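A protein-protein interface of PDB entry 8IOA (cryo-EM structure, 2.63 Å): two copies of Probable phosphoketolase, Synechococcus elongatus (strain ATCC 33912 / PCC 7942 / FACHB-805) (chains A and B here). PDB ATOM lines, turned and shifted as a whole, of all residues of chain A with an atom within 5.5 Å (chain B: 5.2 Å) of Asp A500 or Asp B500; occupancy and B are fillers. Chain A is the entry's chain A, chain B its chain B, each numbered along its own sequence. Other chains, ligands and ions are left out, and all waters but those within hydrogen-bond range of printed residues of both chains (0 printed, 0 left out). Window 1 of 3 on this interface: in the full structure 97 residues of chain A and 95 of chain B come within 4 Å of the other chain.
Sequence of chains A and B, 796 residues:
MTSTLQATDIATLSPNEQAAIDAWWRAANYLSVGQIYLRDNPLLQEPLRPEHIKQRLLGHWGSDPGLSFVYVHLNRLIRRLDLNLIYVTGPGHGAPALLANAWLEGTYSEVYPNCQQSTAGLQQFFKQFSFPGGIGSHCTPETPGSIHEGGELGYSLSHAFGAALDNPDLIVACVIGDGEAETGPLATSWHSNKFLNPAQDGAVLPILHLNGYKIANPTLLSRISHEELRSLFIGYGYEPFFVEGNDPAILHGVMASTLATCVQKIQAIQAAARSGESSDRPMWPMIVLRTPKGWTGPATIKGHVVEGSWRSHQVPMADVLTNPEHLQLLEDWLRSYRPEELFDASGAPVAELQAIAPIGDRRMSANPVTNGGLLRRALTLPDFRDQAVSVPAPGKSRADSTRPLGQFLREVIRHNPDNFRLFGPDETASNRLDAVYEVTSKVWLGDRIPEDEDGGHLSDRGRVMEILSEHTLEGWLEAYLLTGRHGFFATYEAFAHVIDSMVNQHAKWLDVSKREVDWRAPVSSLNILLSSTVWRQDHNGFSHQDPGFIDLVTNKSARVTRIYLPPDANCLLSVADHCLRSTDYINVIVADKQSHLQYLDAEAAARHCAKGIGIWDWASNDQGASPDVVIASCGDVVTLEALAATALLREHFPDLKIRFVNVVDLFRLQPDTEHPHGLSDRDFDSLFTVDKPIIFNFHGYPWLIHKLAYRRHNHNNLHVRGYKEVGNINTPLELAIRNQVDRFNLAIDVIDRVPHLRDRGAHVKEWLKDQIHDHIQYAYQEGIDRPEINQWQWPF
The side-chain carboxylate (OD1) of Asp A500 is in hydrogen-bond range of the side-chain amide nitrogen (ND2) of Asn A504, 3.3 Å away.
His A497 touches Asn B504, but with the chains exchanged Asn A504 does not touch His B497 (4.2 Å).
Asp A500 touches His B497, but with the chains exchanged His A497 does not touch Asp B500 (4.9 Å).
Asp A500 touches its own counterpart, Asp B500.
Asp A500 touches Leu B552, but with the chains exchanged Leu A552 does not touch Asp B500 (4.3 Å).
Positions printed for both chains: 496, 497, 498, 499, 500, 501, 502, 503, 504, 549 and 552.
Of the 7 pairs that touch across the chains among the printed residues, 4 have their exchanged pair printed and touching as well.
Printed residues of chain B within 4 Å of His A497: Asn B504 and Leu B552.
Printed residues of chain B within 4 Å of Asp A500: His B497, Asp B500 and Leu B552.
Val A503 touches none of the printed residues of chain B.
Of the printed residues of chain A, His B497 touches Asp A500 and Leu A552.
Printed residues of chain A within 4 Å of Asn B504: His A497 (3.4 Å).
Printed residues of chain A within 4 Å of Leu B552: His A497 (3.7 Å), Asp A500 (3.97 Å) and Leu A552 (3.9 Å).
The nearest residue of chain A that does not touch Asp B500 is Leu A552 (4.3 Å).
The nearest printed residue of chain A that does not touch His B497 is Ser A501 (4.1 Å).
His A497 touches Leu B552 (CD2 to CD2, 3.7 Å).
His B497 touches Asp A500 (CD2 to OD2, 3.4 Å).
Leu B552 touches Asp A500 (CD2 to OD2, 3.97 Å).
Leu A552 touches His B497 (CD1 to NE2, 3.5 Å).
Leu A552 touches Leu B552.
Hydrophobic or aromatic side chains of chain B within 4 Å of the printed part of chain A: His B497 and Leu B552.
Printed residues of chain A that touch a printed residue of chain B: His A497, Asp A500 and Leu A552.
Along chain A the printed residues that touch a printed residue of chain B span positions 497 to 552.
Among the printed residues, no Asp or Glu carboxylate lies within 4 Å of a Lys or Arg side-chain nitrogen of the other chain.
OD2 of Asp A500 lies close to OD2 of Asp B500, at 2.9 Å.
A ring nitrogen (NE2) of His A497 sits at hydrogen-bond distance from the side-chain amide nitrogen (ND2) of Asn B504.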
ATOM      1  N   ALA A 496      25.840  -3.688 -15.100  1.00  0.00           N
ATOM      2  CA  ALA A 496      26.650  -2.615 -14.550  1.00  0.00           C
ATOM      3  C   ALA A 496      25.829  -1.618 -13.749  1.00  0.00           C
ATOM      4  O   ALA A 496      26.396  -0.883 -12.935  1.00  0.00           O
ATOM      5  CB  ALA A 496      27.392  -1.894 -15.674  1.00  0.00           C
ATOM      6  N   HIS A 497      24.514  -1.571 -13.959  1.00  0.00           N
ATOM      7  CA  HIS A 497      23.659  -0.724 -13.139  1.00  0.00           C
ATOM      8  C   HIS A 497      23.586  -1.204 -11.698  1.00  0.00           C
ATOM      9  O   HIS A 497      23.195  -0.431 -10.820  1.00  0.00           O
ATOM     10  CB  HIS A 497      22.251  -0.665 -13.724  1.00  0.00           C
ATOM     11  CG  HIS A 497      22.099   0.324 -14.834  1.00  0.00           C
ATOM     12  ND1 HIS A 497      22.045  -0.047 -16.159  1.00  0.00           N
ATOM     13  CD2 HIS A 497      21.990   1.673 -14.815  1.00  0.00           C
ATOM     14  CE1 HIS A 497      21.907   1.032 -16.910  1.00  0.00           C
ATOM     15  NE2 HIS A 497      21.871   2.088 -16.119  1.00  0.00           N
ATOM     16  N   VAL A 498      23.931  -2.463 -11.441  1.00  0.00           N
ATOM     17  CA  VAL A 498      23.878  -2.987 -10.083  1.00  0.00           C
ATOM     18  C   VAL A 498      24.960  -2.357  -9.218  1.00  0.00           C
ATOM     19  O   VAL A 498      24.722  -2.010  -8.057  1.00  0.00           O
ATOM     20  CB  VAL A 498      23.997  -4.518 -10.106  1.00  0.00           C
ATOM     21  CG1 VAL A 498      24.003  -5.069  -8.697  1.00  0.00           C
ATOM     22  CG2 VAL A 498      22.867  -5.116 -10.913  1.00  0.00           C
ATOM     23  N   ILE A 499      26.161  -2.201  -9.763  1.00  0.00           N
ATOM     24  CA  ILE A 499      27.286  -1.675  -8.998  1.00  0.00           C
ATOM     25  C   ILE A 499      27.337  -0.168  -9.167  1.00  0.00           C
ATOM     26  O   ILE A 499      28.368   0.464  -8.920  1.00  0.00           O
ATOM     27  CB  ILE A 499      28.608  -2.321  -9.435  1.00  0.00           C
ATOM     28  CG1 ILE A 499      28.901  -1.994 -10.896  1.00  0.00           C
ATOM     29  CG2 ILE A 499      28.547  -3.814  -9.241  1.00  0.00           C
ATOM     30  CD1 ILE A 499      30.222  -2.527 -11.376  1.00  0.00           C
ATOM     31  N   ASP A 500      26.220   0.413  -9.598  1.00  0.00           N
ATOM     32  CA  ASP A 500      26.169   1.841  -9.878  1.00  0.00           C
ATOM     33  C   ASP A 500      26.510   2.665  -8.643  1.00  0.00           C
ATOM     34  O   ASP A 500      27.373   3.548  -8.687  1.00  0.00           O
ATOM     35  CB  ASP A 500      24.780   2.200 -10.394  1.00  0.00           C
ATOM     36  CG  ASP A 500      24.706   3.603 -10.911  1.00  0.00           C
ATOM     37  OD1 ASP A 500      25.775   4.232 -11.029  1.00  0.00           O
ATOM     38  OD2 ASP A 500      23.585   4.076 -11.194  1.00  0.00           O
ATOM     39  N   SER A 501      25.838   2.388  -7.527  1.00  0.00           N
ATOM     40  CA  SER A 501      26.055   3.174  -6.320  1.00  0.00           C
ATOM     41  C   SER A 501      27.444   2.943  -5.744  1.00  0.00           C
ATOM     42  O   SER A 501      28.076   3.880  -5.244  1.00  0.00           O
ATOM     43  CB  SER A 501      24.988   2.842  -5.282  1.00  0.00           C
ATOM     44  OG  SER A 501      25.024   1.467  -4.952  1.00  0.00           O
ATOM     45  N   MET A 502      27.933   1.703  -5.790  1.00  0.00           N
ATOM     46  CA  MET A 502      29.227   1.403  -5.191  1.00  0.00           C
ATOM     47  C   MET A 502      30.353   2.128  -5.910  1.00  0.00           C
ATOM     48  O   MET A 502      31.307   2.592  -5.276  1.00  0.00           O
ATOM     49  CB  MET A 502      29.474  -0.102  -5.198  1.00  0.00           C
ATOM     50  CG  MET A 502      28.345  -0.905  -4.606  1.00  0.00           C
ATOM     51  SD  MET A 502      28.823  -2.608  -4.307  1.00  0.00           S
ATOM     52  CE  MET A 502      30.199  -2.366  -3.193  1.00  0.00           C
ATOM     53  N   VAL A 503      30.267   2.226  -7.235  1.00  0.00           N
ATOM     54  CA  VAL A 503      31.311   2.903  -7.996  1.00  0.00           C
ATOM     55  C   VAL A 503      31.371   4.378  -7.626  1.00  0.00           C
ATOM     56  O   VAL A 503      32.455   4.959  -7.508  1.00  0.00           O
ATOM     57  CB  VAL A 503      31.086   2.702  -9.504  1.00  0.00           C
ATOM     58  CG1 VAL A 503      31.990   3.615 -10.300  1.00  0.00           C
ATOM     59  CG2 VAL A 503      31.343   1.259  -9.874  1.00  0.00           C
ATOM     60  N   ASN A 504      30.212   5.008  -7.432  1.00  0.00           N
ATOM     61  CA  ASN A 504      30.200   6.413  -7.041  1.00  0.00           C
ATOM     62  C   ASN A 504      30.869   6.616  -5.691  1.00  0.00           C
ATOM     63  O   ASN A 504      31.607   7.587  -5.496  1.00  0.00           O
ATOM     64  CB  ASN A 504      28.770   6.944  -7.012  1.00  0.00           C
ATOM     65  CG  ASN A 504      28.125   6.947  -8.376  1.00  0.00           C
ATOM     66  OD1 ASN A 504      28.255   7.904  -9.135  1.00  0.00           O
ATOM     67  ND2 ASN A 504      27.422   5.871  -8.698  1.00  0.00           N
ATOM     68  N   PHE A 549      25.483   2.768 -18.163  1.00  0.00           N
ATOM     69  CA  PHE A 549      26.555   2.822 -17.176  1.00  0.00           C
ATOM     70  C   PHE A 549      27.711   3.679 -17.668  1.00  0.00           C
ATOM     71  O   PHE A 549      28.354   4.377 -16.878  1.00  0.00           O
ATOM     72  CB  PHE A 549      27.043   1.418 -16.839  1.00  0.00           C
ATOM     73  CG  PHE A 549      28.171   1.395 -15.848  1.00  0.00           C
ATOM     74  CD1 PHE A 549      27.926   1.549 -14.497  1.00  0.00           C
ATOM     75  CD2 PHE A 549      29.476   1.214 -16.267  1.00  0.00           C
ATOM     76  CE1 PHE A 549      28.959   1.528 -13.586  1.00  0.00           C
ATOM     77  CE2 PHE A 549      30.511   1.191 -15.359  1.00  0.00           C
ATOM     78  CZ  PHE A 549      30.253   1.348 -14.018  1.00  0.00           C
ATOM     79  N   LEU A 552      26.865   7.247 -16.836  1.00  0.00           N
ATOM     80  CA  LEU A 552      26.933   7.642 -15.435  1.00  0.00           C
ATOM     81  C   LEU A 552      28.366   7.901 -14.996  1.00  0.00           C
ATOM     82  O   LEU A 552      28.630   8.857 -14.260  1.00  0.00           O
ATOM     83  CB  LEU A 552      26.294   6.578 -14.549  1.00  0.00           C
ATOM     84  CG  LEU A 552      26.047   7.096 -13.134  1.00  0.00           C
ATOM     85  CD1 LEU A 552      24.685   6.649 -12.641  1.00  0.00           C
ATOM     86  CD2 LEU A 552      27.155   6.668 -12.174  1.00  0.00           C
ATOM     87  N   ALA B 496      18.863   7.408  -4.439  1.00  0.00           N
ATOM     88  CA  ALA B 496      18.141   7.032  -5.643  1.00  0.00           C
ATOM     89  C   ALA B 496      18.977   6.177  -6.582  1.00  0.00           C
ATOM     90  O   ALA B 496      18.413   5.495  -7.442  1.00  0.00           O
ATOM     91  CB  ALA B 496      17.657   8.282  -6.372  1.00  0.00           C
ATOM     92  N   HIS B 497      20.303   6.201  -6.444  1.00  0.00           N
ATOM     93  CA  HIS B 497      21.144   5.312  -7.232  1.00  0.00           C
ATOM     94  C   HIS B 497      20.940   3.852  -6.865  1.00  0.00           C
ATOM     95  O   HIS B 497      21.271   2.973  -7.665  1.00  0.00           O
ATOM     96  CB  HIS B 497      22.615   5.680  -7.056  1.00  0.00           C
ATOM     97  CG  HIS B 497      23.072   6.794  -7.943  1.00  0.00           C
ATOM     98  ND1 HIS B 497      23.288   8.073  -7.481  1.00  0.00           N
ATOM     99  CD2 HIS B 497      23.352   6.818  -9.266  1.00  0.00           C
ATOM    100  CE1 HIS B 497      23.685   8.837  -8.483  1.00  0.00           C
ATOM    101  NE2 HIS B 497      23.731   8.100  -9.577  1.00  0.00           N
ATOM    102  N   VAL B 498      20.408   3.578  -5.675  1.00  0.00           N
ATOM    103  CA  VAL B 498      20.207   2.199  -5.249  1.00  0.00           C
ATOM    104  C   VAL B 498      19.137   1.523  -6.095  1.00  0.00           C
ATOM    105  O   VAL B 498      19.289   0.368  -6.505  1.00  0.00           O
ATOM    106  CB  VAL B 498      19.858   2.157  -3.752  1.00  0.00           C
ATOM    107  CG1 VAL B 498      19.569   0.739  -3.317  1.00  0.00           C
ATOM    108  CG2 VAL B 498      20.989   2.748  -2.936  1.00  0.00           C
ATOM    109  N   ILE B 499      18.044   2.227  -6.375  1.00  0.00           N
ATOM    110  CA  ILE B 499      16.913   1.640  -7.083  1.00  0.00           C
ATOM    111  C   ILE B 499      17.045   1.909  -8.573  1.00  0.00           C
ATOM    112  O   ILE B 499      16.074   1.783  -9.325  1.00  0.00           O
ATOM    113  CB  ILE B 499      15.580   2.186  -6.547  1.00  0.00           C
ATOM    114  CG1 ILE B 499      15.475   3.684  -6.822  1.00  0.00           C
ATOM    115  CG2 ILE B 499      15.459   1.917  -5.066  1.00  0.00           C
ATOM    116  CD1 ILE B 499      14.186   4.294  -6.348  1.00  0.00           C
ATOM    117  N   ASP B 500      18.247   2.283  -9.008  1.00  0.00           N
ATOM    118  CA  ASP B 500      18.450   2.647 -10.405  1.00  0.00           C
ATOM    119  C   ASP B 500      18.155   1.477 -11.333  1.00  0.00           C
ATOM    120  O   ASP B 500      17.480   1.635 -12.356  1.00  0.00           O
ATOM    121  CB  ASP B 500      19.878   3.142 -10.606  1.00  0.00           C
ATOM    122  CG  ASP B 500      19.937   4.441 -11.368  1.00  0.00           C
ATOM    123  OD1 ASP B 500      19.028   4.688 -12.187  1.00  0.00           O
ATOM    124  OD2 ASP B 500      20.889   5.218 -11.145  1.00  0.00           O
ATOM    125  N   SER B 501      18.661   0.291 -10.998  1.00  0.00           N
ATOM    126  CA  SER B 501      18.426  -0.873 -11.844  1.00  0.00           C
ATOM    127  C   SER B 501      16.957  -1.271 -11.846  1.00  0.00           C
ATOM    128  O   SER B 501      16.413  -1.647 -12.890  1.00  0.00           O
ATOM    129  CB  SER B 501      19.296  -2.040 -11.385  1.00  0.00           C
ATOM    130  OG  SER B 501      19.021  -2.377 -10.040  1.00  0.00           O
ATOM    131  N   MET B 502      16.300  -1.203 -10.688  1.00  0.00           N
ATOM    132  CA  MET B 502      14.900  -1.606 -10.608  1.00  0.00           C
ATOM    133  C   MET B 502      14.009  -0.690 -11.434  1.00  0.00           C
ATOM    134  O   MET B 502      13.053  -1.152 -12.065  1.00  0.00           O
ATOM    135  CB  MET B 502      14.442  -1.624  -9.154  1.00  0.00           C
ATOM    136  CG  MET B 502      15.329  -2.436  -8.243  1.00  0.00           C
ATOM    137  SD  MET B 502      14.562  -2.723  -6.646  1.00  0.00           S
ATOM    138  CE  MET B 502      13.102  -3.624  -7.146  1.00  0.00           C
ATOM    139  N   VAL B 503      14.294   0.611 -11.430  1.00  0.00           N
ATOM    140  CA  VAL B 503      13.489   1.547 -12.207  1.00  0.00           C
ATOM    141  C   VAL B 503      13.611   1.249 -13.693  1.00  0.00           C
ATOM    142  O   VAL B 503      12.629   1.332 -14.440  1.00  0.00           O
ATOM    143  CB  VAL B 503      13.889   2.996 -11.880  1.00  0.00           C
ATOM    144  CG1 VAL B 503      13.233   3.955 -12.847  1.00  0.00           C
ATOM    145  CG2 VAL B 503      13.494   3.333 -10.461  1.00  0.00           C
ATOM    146  N   ASN B 504      14.813   0.894 -14.150  1.00  0.00           N
ATOM    147  CA  ASN B 504      14.988   0.543 -15.555  1.00  0.00           C
ATOM    148  C   ASN B 504      14.151  -0.669 -15.930  1.00  0.00           C
ATOM    149  O   ASN B 504      13.544  -0.703 -17.005  1.00  0.00           O
ATOM    150  CB  ASN B 504      16.461   0.285 -15.858  1.00  0.00           C
ATOM    151  CG  ASN B 504      17.281   1.551 -15.863  1.00  0.00           C
ATOM    152  OD1 ASN B 504      16.746   2.649 -15.998  1.00  0.00           O
ATOM    153  ND2 ASN B 504      18.592   1.407 -15.724  1.00  0.00           N
ATOM    154  N   PHE B 549      20.598  10.667 -10.533  1.00  0.00           N
ATOM    155  CA  PHE B 549      19.417   9.855 -10.807  1.00  0.00           C
ATOM    156  C   PHE B 549      18.496  10.541 -11.801  1.00  0.00           C
ATOM    157  O   PHE B 549      17.878   9.882 -12.644  1.00  0.00           O
ATOM    158  CB  PHE B 549      18.666   9.551  -9.516  1.00  0.00           C
ATOM    159  CG  PHE B 549      17.412   8.748  -9.723  1.00  0.00           C
ATOM    160  CD1 PHE B 549      17.476   7.379  -9.906  1.00  0.00           C
ATOM    161  CD2 PHE B 549      16.173   9.359  -9.731  1.00  0.00           C
ATOM    162  CE1 PHE B 549      16.329   6.639 -10.096  1.00  0.00           C
ATOM    163  CE2 PHE B 549      15.024   8.621  -9.920  1.00  0.00           C
ATOM    164  CZ  PHE B 549      15.103   7.260 -10.101  1.00  0.00           C
ATOM    165  N   LEU B 552      19.754   9.720 -15.211  1.00  0.00           N
ATOM    166  CA  LEU B 552      19.601   8.352 -15.690  1.00  0.00           C
ATOM    167  C   LEU B 552      18.164   8.044 -16.084  1.00  0.00           C
ATOM    168  O   LEU B 552      17.933   7.197 -16.953  1.00  0.00           O
ATOM    169  CB  LEU B 552      20.094   7.363 -14.637  1.00  0.00           C
ATOM    170  CG  LEU B 552      20.400   5.964 -15.175  1.00  0.00           C
ATOM    171  CD1 LEU B 552      20.940   6.034 -16.596  1.00  0.00           C
ATOM    172  CD2 LEU B 552      21.402   5.265 -14.284  1.00  0.00           C
